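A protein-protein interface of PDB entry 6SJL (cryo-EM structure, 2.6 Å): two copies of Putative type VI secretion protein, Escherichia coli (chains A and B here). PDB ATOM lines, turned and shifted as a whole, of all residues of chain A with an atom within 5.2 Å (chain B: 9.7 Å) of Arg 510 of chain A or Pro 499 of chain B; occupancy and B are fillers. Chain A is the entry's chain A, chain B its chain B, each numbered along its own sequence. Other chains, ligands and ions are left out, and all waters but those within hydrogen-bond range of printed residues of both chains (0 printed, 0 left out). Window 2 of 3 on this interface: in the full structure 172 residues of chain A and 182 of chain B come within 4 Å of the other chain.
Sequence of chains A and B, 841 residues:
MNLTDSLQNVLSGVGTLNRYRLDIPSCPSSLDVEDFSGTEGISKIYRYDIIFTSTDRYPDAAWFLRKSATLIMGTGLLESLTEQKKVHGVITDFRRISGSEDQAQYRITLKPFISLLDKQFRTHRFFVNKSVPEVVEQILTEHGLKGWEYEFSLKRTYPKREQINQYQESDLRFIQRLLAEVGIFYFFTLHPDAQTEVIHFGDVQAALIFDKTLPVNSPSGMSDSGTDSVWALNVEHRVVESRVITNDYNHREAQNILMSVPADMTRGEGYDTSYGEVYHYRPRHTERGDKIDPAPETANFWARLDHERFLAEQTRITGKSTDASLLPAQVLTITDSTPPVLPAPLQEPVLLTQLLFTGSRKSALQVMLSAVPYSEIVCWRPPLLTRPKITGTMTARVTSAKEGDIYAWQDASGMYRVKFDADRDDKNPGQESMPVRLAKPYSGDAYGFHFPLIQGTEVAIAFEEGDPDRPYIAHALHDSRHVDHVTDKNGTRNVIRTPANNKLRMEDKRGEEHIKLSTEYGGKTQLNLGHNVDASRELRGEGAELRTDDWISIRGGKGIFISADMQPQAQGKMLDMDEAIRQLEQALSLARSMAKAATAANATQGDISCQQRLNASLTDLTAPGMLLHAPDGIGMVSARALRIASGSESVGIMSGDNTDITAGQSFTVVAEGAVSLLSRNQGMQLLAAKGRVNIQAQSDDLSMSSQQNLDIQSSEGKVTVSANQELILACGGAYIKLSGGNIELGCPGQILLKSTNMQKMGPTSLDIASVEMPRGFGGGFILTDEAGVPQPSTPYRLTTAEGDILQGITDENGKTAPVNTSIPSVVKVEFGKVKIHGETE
The side-chain carboxylate (OD2) of Asp 508 of chain A sits close to the side-chain amide oxygen (OD1) of Asn 502 of chain B (2.9 Å).
NH1 of Arg 510 of chain A sits at hydrogen-bond distance from O of Pro 499 of chain B (3.2 Å).
The side-chain hydroxyl of Thr 498 of chain B lies close to the side-chain carboxylate of Asp 508 of chain A (2.4 Å).
OG1 of Thr 498 of chain B sits close to N of Ala 500 of chain B, 3.4 Å away.
The backbone carbonyl oxygen of Asp 508 of chain A lies close to the guanidinium group of Arg 510 of chain A.
OE2 of Glu 513 of chain A is in hydrogen-bond range of N of Gly 511 of chain A.
The side-chain amide nitrogen of Asn 502 of chain B is in hydrogen-bond range of the side-chain hydroxyl of Thr 519 of chain B.
The side-chain hydroxyl (OG1) of Thr 498 of chain B sits at hydrogen-bond distance from the backbone NH (N) of Asn 502 of chain B (3.3 Å).
Among the printed residues, merely in contact across the chains: Gly 511 of chain A with Tyr 521 of chain B (3.1 Å), Glu 513 of chain A with Tyr 521 of chain B (3.2 Å), Asp 508 of chain A with Ala 500 of chain B (3.4 Å), Glu 513 of chain A with Thr 519 of chain B (3.4 Å), Glu 513 of chain A with Asn 502 of chain B (3.6 Å), Glu 513 of chain A with Ala 500 of chain B (3.7 Å) and Arg 510 of chain A with Ala 500 of chain B (3.9 Å).
Of the printed residues of chain B, Gly 511 of chain A touches Tyr 521.
Of the printed residues of chain A, Thr 498 of chain B touches Asp 508.
Pro 499 of chain B touches just one residue of chain A: Arg 510 (3.2 Å).
Asn 501 of chain B touches none of the printed residues of chain A.
Printed residues of chain A within 4 Å of Asn 502 of chain B: Asp 508 and Glu 513.
Of the printed residues of chain A, Thr 519 of chain B touches Glu 513 (3.4 Å).
Printed residues of chain A within 4 Å of Tyr 521 of chain B: Gly 511 (3.1 Å) and Glu 513 (3.2 Å).
The nearest residue of chain B that does not touch Arg 510 of chain A is Asn 501 of chain B (6.2 Å).
The nearest residue of chain A that does not touch Pro 499 of chain B is Asp 508 of chain A (4.6 Å).
The nearest printed residue of chain A that does not touch Asn 502 of chain B is Lys 509 of chain A (5.9 Å).
Of the 11 printed residues of chain B, 6 touch a printed residue of chain A.
Hydrophobic or aromatic side chains of chain B within 4 Å of the printed part of chain A: Pro 499, Ala 500 and Tyr 521.
Among the printed residues, no Asp or Glu carboxylate lies within 4 Å of a Lys or Arg side-chain nitrogen of the other chain.
No position is printed for both chains.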
ATOM      1  N   ASP A 508     -13.558 -14.502   2.768  1.00  0.00           N
ATOM      2  CA  ASP A 508     -12.536 -13.566   2.330  1.00  0.00           C
ATOM      3  C   ASP A 508     -12.817 -12.132   2.715  1.00  0.00           C
ATOM      4  O   ASP A 508     -12.066 -11.251   2.307  1.00  0.00           O
ATOM      5  CB  ASP A 508     -12.349 -13.626   0.823  1.00  0.00           C
ATOM      6  CG  ASP A 508     -12.007 -14.985   0.350  1.00  0.00           C
ATOM      7  OD1 ASP A 508     -12.690 -15.474  -0.562  1.00  0.00           O
ATOM      8  OD2 ASP A 508     -11.059 -15.568   0.900  1.00  0.00           O
ATOM      9  N   LYS A 509     -13.878 -11.871   3.457  1.00  0.00           N
ATOM     10  CA  LYS A 509     -14.137 -10.522   3.916  1.00  0.00           C
ATOM     11  C   LYS A 509     -12.907 -10.003   4.621  1.00  0.00           C
ATOM     12  O   LYS A 509     -12.475 -10.580   5.615  1.00  0.00           O
ATOM     13  CB  LYS A 509     -15.337 -10.508   4.847  1.00  0.00           C
ATOM     14  CG  LYS A 509     -15.819  -9.134   5.175  1.00  0.00           C
ATOM     15  CD  LYS A 509     -16.889  -9.176   6.218  1.00  0.00           C
ATOM     16  CE  LYS A 509     -17.303  -7.781   6.609  1.00  0.00           C
ATOM     17  NZ  LYS A 509     -18.445  -7.806   7.545  1.00  0.00           N
ATOM     18  N   ARG A 510     -12.312  -8.946   4.079  1.00  0.00           N
ATOM     19  CA  ARG A 510     -11.034  -8.479   4.592  1.00  0.00           C
ATOM     20  C   ARG A 510     -11.172  -8.020   6.028  1.00  0.00           C
ATOM     21  O   ARG A 510     -12.169  -7.410   6.408  1.00  0.00           O
ATOM     22  CB  ARG A 510     -10.494  -7.348   3.736  1.00  0.00           C
ATOM     23  CG  ARG A 510      -9.517  -7.784   2.687  1.00  0.00           C
ATOM     24  CD  ARG A 510     -10.209  -8.561   1.621  1.00  0.00           C
ATOM     25  NE  ARG A 510      -9.371  -8.739   0.449  1.00  0.00           N
ATOM     26  CZ  ARG A 510      -9.753  -9.395  -0.633  1.00  0.00           C
ATOM     27  NH1 ARG A 510      -8.938  -9.497  -1.666  1.00  0.00           N
ATOM     28  NH2 ARG A 510     -10.956  -9.941  -0.681  1.00  0.00           N
ATOM     29  N   GLY A 511     -10.162  -8.322   6.833  1.00  0.00           N
ATOM     30  CA  GLY A 511     -10.235  -8.072   8.247  1.00  0.00           C
ATOM     31  C   GLY A 511     -11.135  -9.007   9.000  1.00  0.00           C
ATOM     32  O   GLY A 511     -11.158  -8.957  10.229  1.00  0.00           O
ATOM     33  N   GLU A 512     -11.880  -9.853   8.308  1.00  0.00           N
ATOM     34  CA  GLU A 512     -12.781 -10.816   8.912  1.00  0.00           C
ATOM     35  C   GLU A 512     -12.667 -12.162   8.224  1.00  0.00           C
ATOM     36  O   GLU A 512     -13.660 -12.877   8.087  1.00  0.00           O
ATOM     37  CB  GLU A 512     -14.215 -10.332   8.841  1.00  0.00           C
ATOM     38  CG  GLU A 512     -14.452  -9.081   9.606  1.00  0.00           C
ATOM     39  CD  GLU A 512     -15.900  -8.882   9.918  1.00  0.00           C
ATOM     40  OE1 GLU A 512     -16.723  -9.669   9.422  1.00  0.00           O
ATOM     41  OE2 GLU A 512     -16.222  -7.943  10.668  1.00  0.00           O
ATOM     42  N   GLU A 513     -11.477 -12.508   7.759  1.00  0.00           N
ATOM     43  CA  GLU A 513     -11.284 -13.765   7.067  1.00  0.00           C
ATOM     44  C   GLU A 513     -11.314 -14.932   8.035  1.00  0.00           C
ATOM     45  O   GLU A 513     -10.839 -14.843   9.162  1.00  0.00           O
ATOM     46  CB  GLU A 513      -9.960 -13.765   6.325  1.00  0.00           C
ATOM     47  CG  GLU A 513      -9.681 -12.541   5.529  1.00  0.00           C
ATOM     48  CD  GLU A 513      -8.743 -11.617   6.225  1.00  0.00           C
ATOM     49  OE1 GLU A 513      -8.623 -11.724   7.448  1.00  0.00           O
ATOM     50  OE2 GLU A 513      -8.091 -10.801   5.552  1.00  0.00           O
ATOM     51  N   ILE B 496      -4.989 -23.989  -2.988  1.00  0.00           N
ATOM     52  CA  ILE B 496      -6.301 -23.370  -3.091  1.00  0.00           C
ATOM     53  C   ILE B 496      -6.225 -22.048  -2.349  1.00  0.00           C
ATOM     54  O   ILE B 496      -6.395 -22.009  -1.132  1.00  0.00           O
ATOM     55  CB  ILE B 496      -7.386 -24.279  -2.501  1.00  0.00           C
ATOM     56  CG1 ILE B 496      -7.498 -25.549  -3.327  1.00  0.00           C
ATOM     57  CG2 ILE B 496      -8.704 -23.555  -2.404  1.00  0.00           C
ATOM     58  CD1 ILE B 496      -8.271 -26.631  -2.636  1.00  0.00           C
ATOM     59  N   ARG B 497      -5.944 -20.965  -3.061  1.00  0.00           N
ATOM     60  CA  ARG B 497      -5.662 -19.676  -2.449  1.00  0.00           C
ATOM     61  C   ARG B 497      -6.692 -18.656  -2.893  1.00  0.00           C
ATOM     62  O   ARG B 497      -6.955 -18.517  -4.087  1.00  0.00           O
ATOM     63  CB  ARG B 497      -4.264 -19.195  -2.814  1.00  0.00           C
ATOM     64  CG  ARG B 497      -3.753 -18.091  -1.933  1.00  0.00           C
ATOM     65  CD  ARG B 497      -2.751 -17.244  -2.669  1.00  0.00           C
ATOM     66  NE  ARG B 497      -2.626 -15.918  -2.079  1.00  0.00           N
ATOM     67  CZ  ARG B 497      -3.197 -14.826  -2.574  1.00  0.00           C
ATOM     68  NH1 ARG B 497      -3.936 -14.901  -3.669  1.00  0.00           N
ATOM     69  NH2 ARG B 497      -3.029 -13.658  -1.973  1.00  0.00           N
ATOM     70  N   THR B 498      -7.257 -17.951  -1.945  1.00  0.00           N
ATOM     71  CA  THR B 498      -8.252 -16.943  -2.225  1.00  0.00           C
ATOM     72  C   THR B 498      -7.629 -15.560  -2.168  1.00  0.00           C
ATOM     73  O   THR B 498      -6.549 -15.378  -1.604  1.00  0.00           O
ATOM     74  CB  THR B 498      -9.403 -17.036  -1.227  1.00  0.00           C
ATOM     75  OG1 THR B 498      -9.048 -16.358  -0.025  1.00  0.00           O
ATOM     76  CG2 THR B 498      -9.711 -18.470  -0.906  1.00  0.00           C
ATOM     77  N   PRO B 499      -8.272 -14.558  -2.770  1.00  0.00           N
ATOM     78  CA  PRO B 499      -7.680 -13.215  -2.782  1.00  0.00           C
ATOM     79  C   PRO B 499      -7.432 -12.625  -1.408  1.00  0.00           C
ATOM     80  O   PRO B 499      -6.604 -11.721  -1.277  1.00  0.00           O
ATOM     81  CB  PRO B 499      -8.704 -12.395  -3.573  1.00  0.00           C
ATOM     82  CG  PRO B 499      -9.874 -13.261  -3.751  1.00  0.00           C
ATOM     83  CD  PRO B 499      -9.413 -14.648  -3.686  1.00  0.00           C
ATOM     84  N   ALA B 500      -8.126 -13.095  -0.381  1.00  0.00           N
ATOM     85  CA  ALA B 500      -7.827 -12.704   0.987  1.00  0.00           C
ATOM     86  C   ALA B 500      -6.719 -13.528   1.599  1.00  0.00           C
ATOM     87  O   ALA B 500      -6.461 -13.384   2.794  1.00  0.00           O
ATOM     88  CB  ALA B 500      -9.070 -12.814   1.857  1.00  0.00           C
ATOM     89  N   ASN B 501      -6.071 -14.382   0.809  1.00  0.00           N
ATOM     90  CA  ASN B 501      -4.964 -15.214   1.259  1.00  0.00           C
ATOM     91  C   ASN B 501      -5.407 -16.244   2.288  1.00  0.00           C
ATOM     92  O   ASN B 501      -4.639 -16.623   3.171  1.00  0.00           O
ATOM     93  CB  ASN B 501      -3.815 -14.368   1.802  1.00  0.00           C
ATOM     94  CG  ASN B 501      -2.469 -15.007   1.584  1.00  0.00           C
ATOM     95  OD1 ASN B 501      -2.248 -15.685   0.593  1.00  0.00           O
ATOM     96  ND2 ASN B 501      -1.561 -14.794   2.511  1.00  0.00           N
ATOM     97  N   ASN B 502      -6.650 -16.694   2.197  1.00  0.00           N
ATOM     98  CA  ASN B 502      -7.047 -17.946   2.817  1.00  0.00           C
ATOM     99  C   ASN B 502      -6.573 -19.047   1.895  1.00  0.00           C
ATOM    100  O   ASN B 502      -7.016 -19.128   0.752  1.00  0.00           O
ATOM    101  CB  ASN B 502      -8.555 -18.033   2.995  1.00  0.00           C
ATOM    102  CG  ASN B 502      -9.096 -16.966   3.846  1.00  0.00           C
ATOM    103  OD1 ASN B 502     -10.097 -16.366   3.522  1.00  0.00           O
ATOM    104  ND2 ASN B 502      -8.440 -16.702   4.944  1.00  0.00           N
ATOM    105  N   LYS B 503      -5.673 -19.886   2.359  1.00  0.00           N
ATOM    106  CA  LYS B 503      -5.085 -20.865   1.475  1.00  0.00           C
ATOM    107  C   LYS B 503      -5.164 -22.243   2.092  1.00  0.00           C
ATOM    108  O   LYS B 503      -5.154 -22.400   3.309  1.00  0.00           O
ATOM    109  CB  LYS B 503      -3.647 -20.527   1.152  1.00  0.00           C
ATOM    110  CG  LYS B 503      -2.841 -20.171   2.335  1.00  0.00           C
ATOM    111  CD  LYS B 503      -1.400 -20.099   1.976  1.00  0.00           C
ATOM    112  CE  LYS B 503      -1.129 -18.884   1.149  1.00  0.00           C
ATOM    113  NZ  LYS B 503       0.314 -18.764   0.852  1.00  0.00           N
ATOM    114  N   THR B 519      -5.182 -18.758   7.352  1.00  0.00           N
ATOM    115  CA  THR B 519      -5.938 -17.539   7.139  1.00  0.00           C
ATOM    116  C   THR B 519      -5.120 -16.388   7.689  1.00  0.00           C
ATOM    117  O   THR B 519      -4.266 -16.576   8.548  1.00  0.00           O
ATOM    118  CB  THR B 519      -7.338 -17.590   7.784  1.00  0.00           C
ATOM    119  OG1 THR B 519      -8.076 -16.440   7.389  1.00  0.00           O
ATOM    120  CG2 THR B 519      -7.268 -17.611   9.260  1.00  0.00           C
ATOM    121  N   GLU B 520      -5.347 -15.200   7.143  1.00  0.00           N
ATOM    122  CA  GLU B 520      -4.591 -14.038   7.580  1.00  0.00           C
ATOM    123  C   GLU B 520      -5.061 -13.512   8.918  1.00  0.00           C
ATOM    124  O   GLU B 520      -4.266 -12.943   9.659  1.00  0.00           O
ATOM    125  CB  GLU B 520      -4.682 -12.934   6.542  1.00  0.00           C
ATOM    126  CG  GLU B 520      -3.749 -13.110   5.404  1.00  0.00           C
ATOM    127  CD  GLU B 520      -2.330 -13.251   5.864  1.00  0.00           C
ATOM    128  OE1 GLU B 520      -1.890 -12.439   6.700  1.00  0.00           O
ATOM    129  OE2 GLU B 520      -1.642 -14.174   5.398  1.00  0.00           O
ATOM    130  N   TYR B 521      -6.329 -13.690   9.243  1.00  0.00           N
ATOM    131  CA  TYR B 521      -6.864 -13.126  10.465  1.00  0.00           C
ATOM    132  C   TYR B 521      -6.148 -13.686  11.676  1.00  0.00           C
ATOM    133  O   TYR B 521      -5.818 -14.869  11.729  1.00  0.00           O
ATOM    134  CB  TYR B 521      -8.352 -13.414  10.565  1.00  0.00           C
ATOM    135  CG  TYR B 521      -9.031 -12.687  11.685  1.00  0.00           C
ATOM    136  CD1 TYR B 521      -9.047 -13.208  12.961  1.00  0.00           C
ATOM    137  CD2 TYR B 521      -9.640 -11.488  11.476  1.00  0.00           C
ATOM    138  CE1 TYR B 521      -9.653 -12.557  13.976  1.00  0.00           C
ATOM    139  CE2 TYR B 521     -10.250 -10.832  12.487  1.00  0.00           C
ATOM    140  CZ  TYR B 521     -10.253 -11.365  13.733  1.00  0.00           C
ATOM    141  OH  TYR B 521     -10.872 -10.683  14.742  1.00  0.00           O
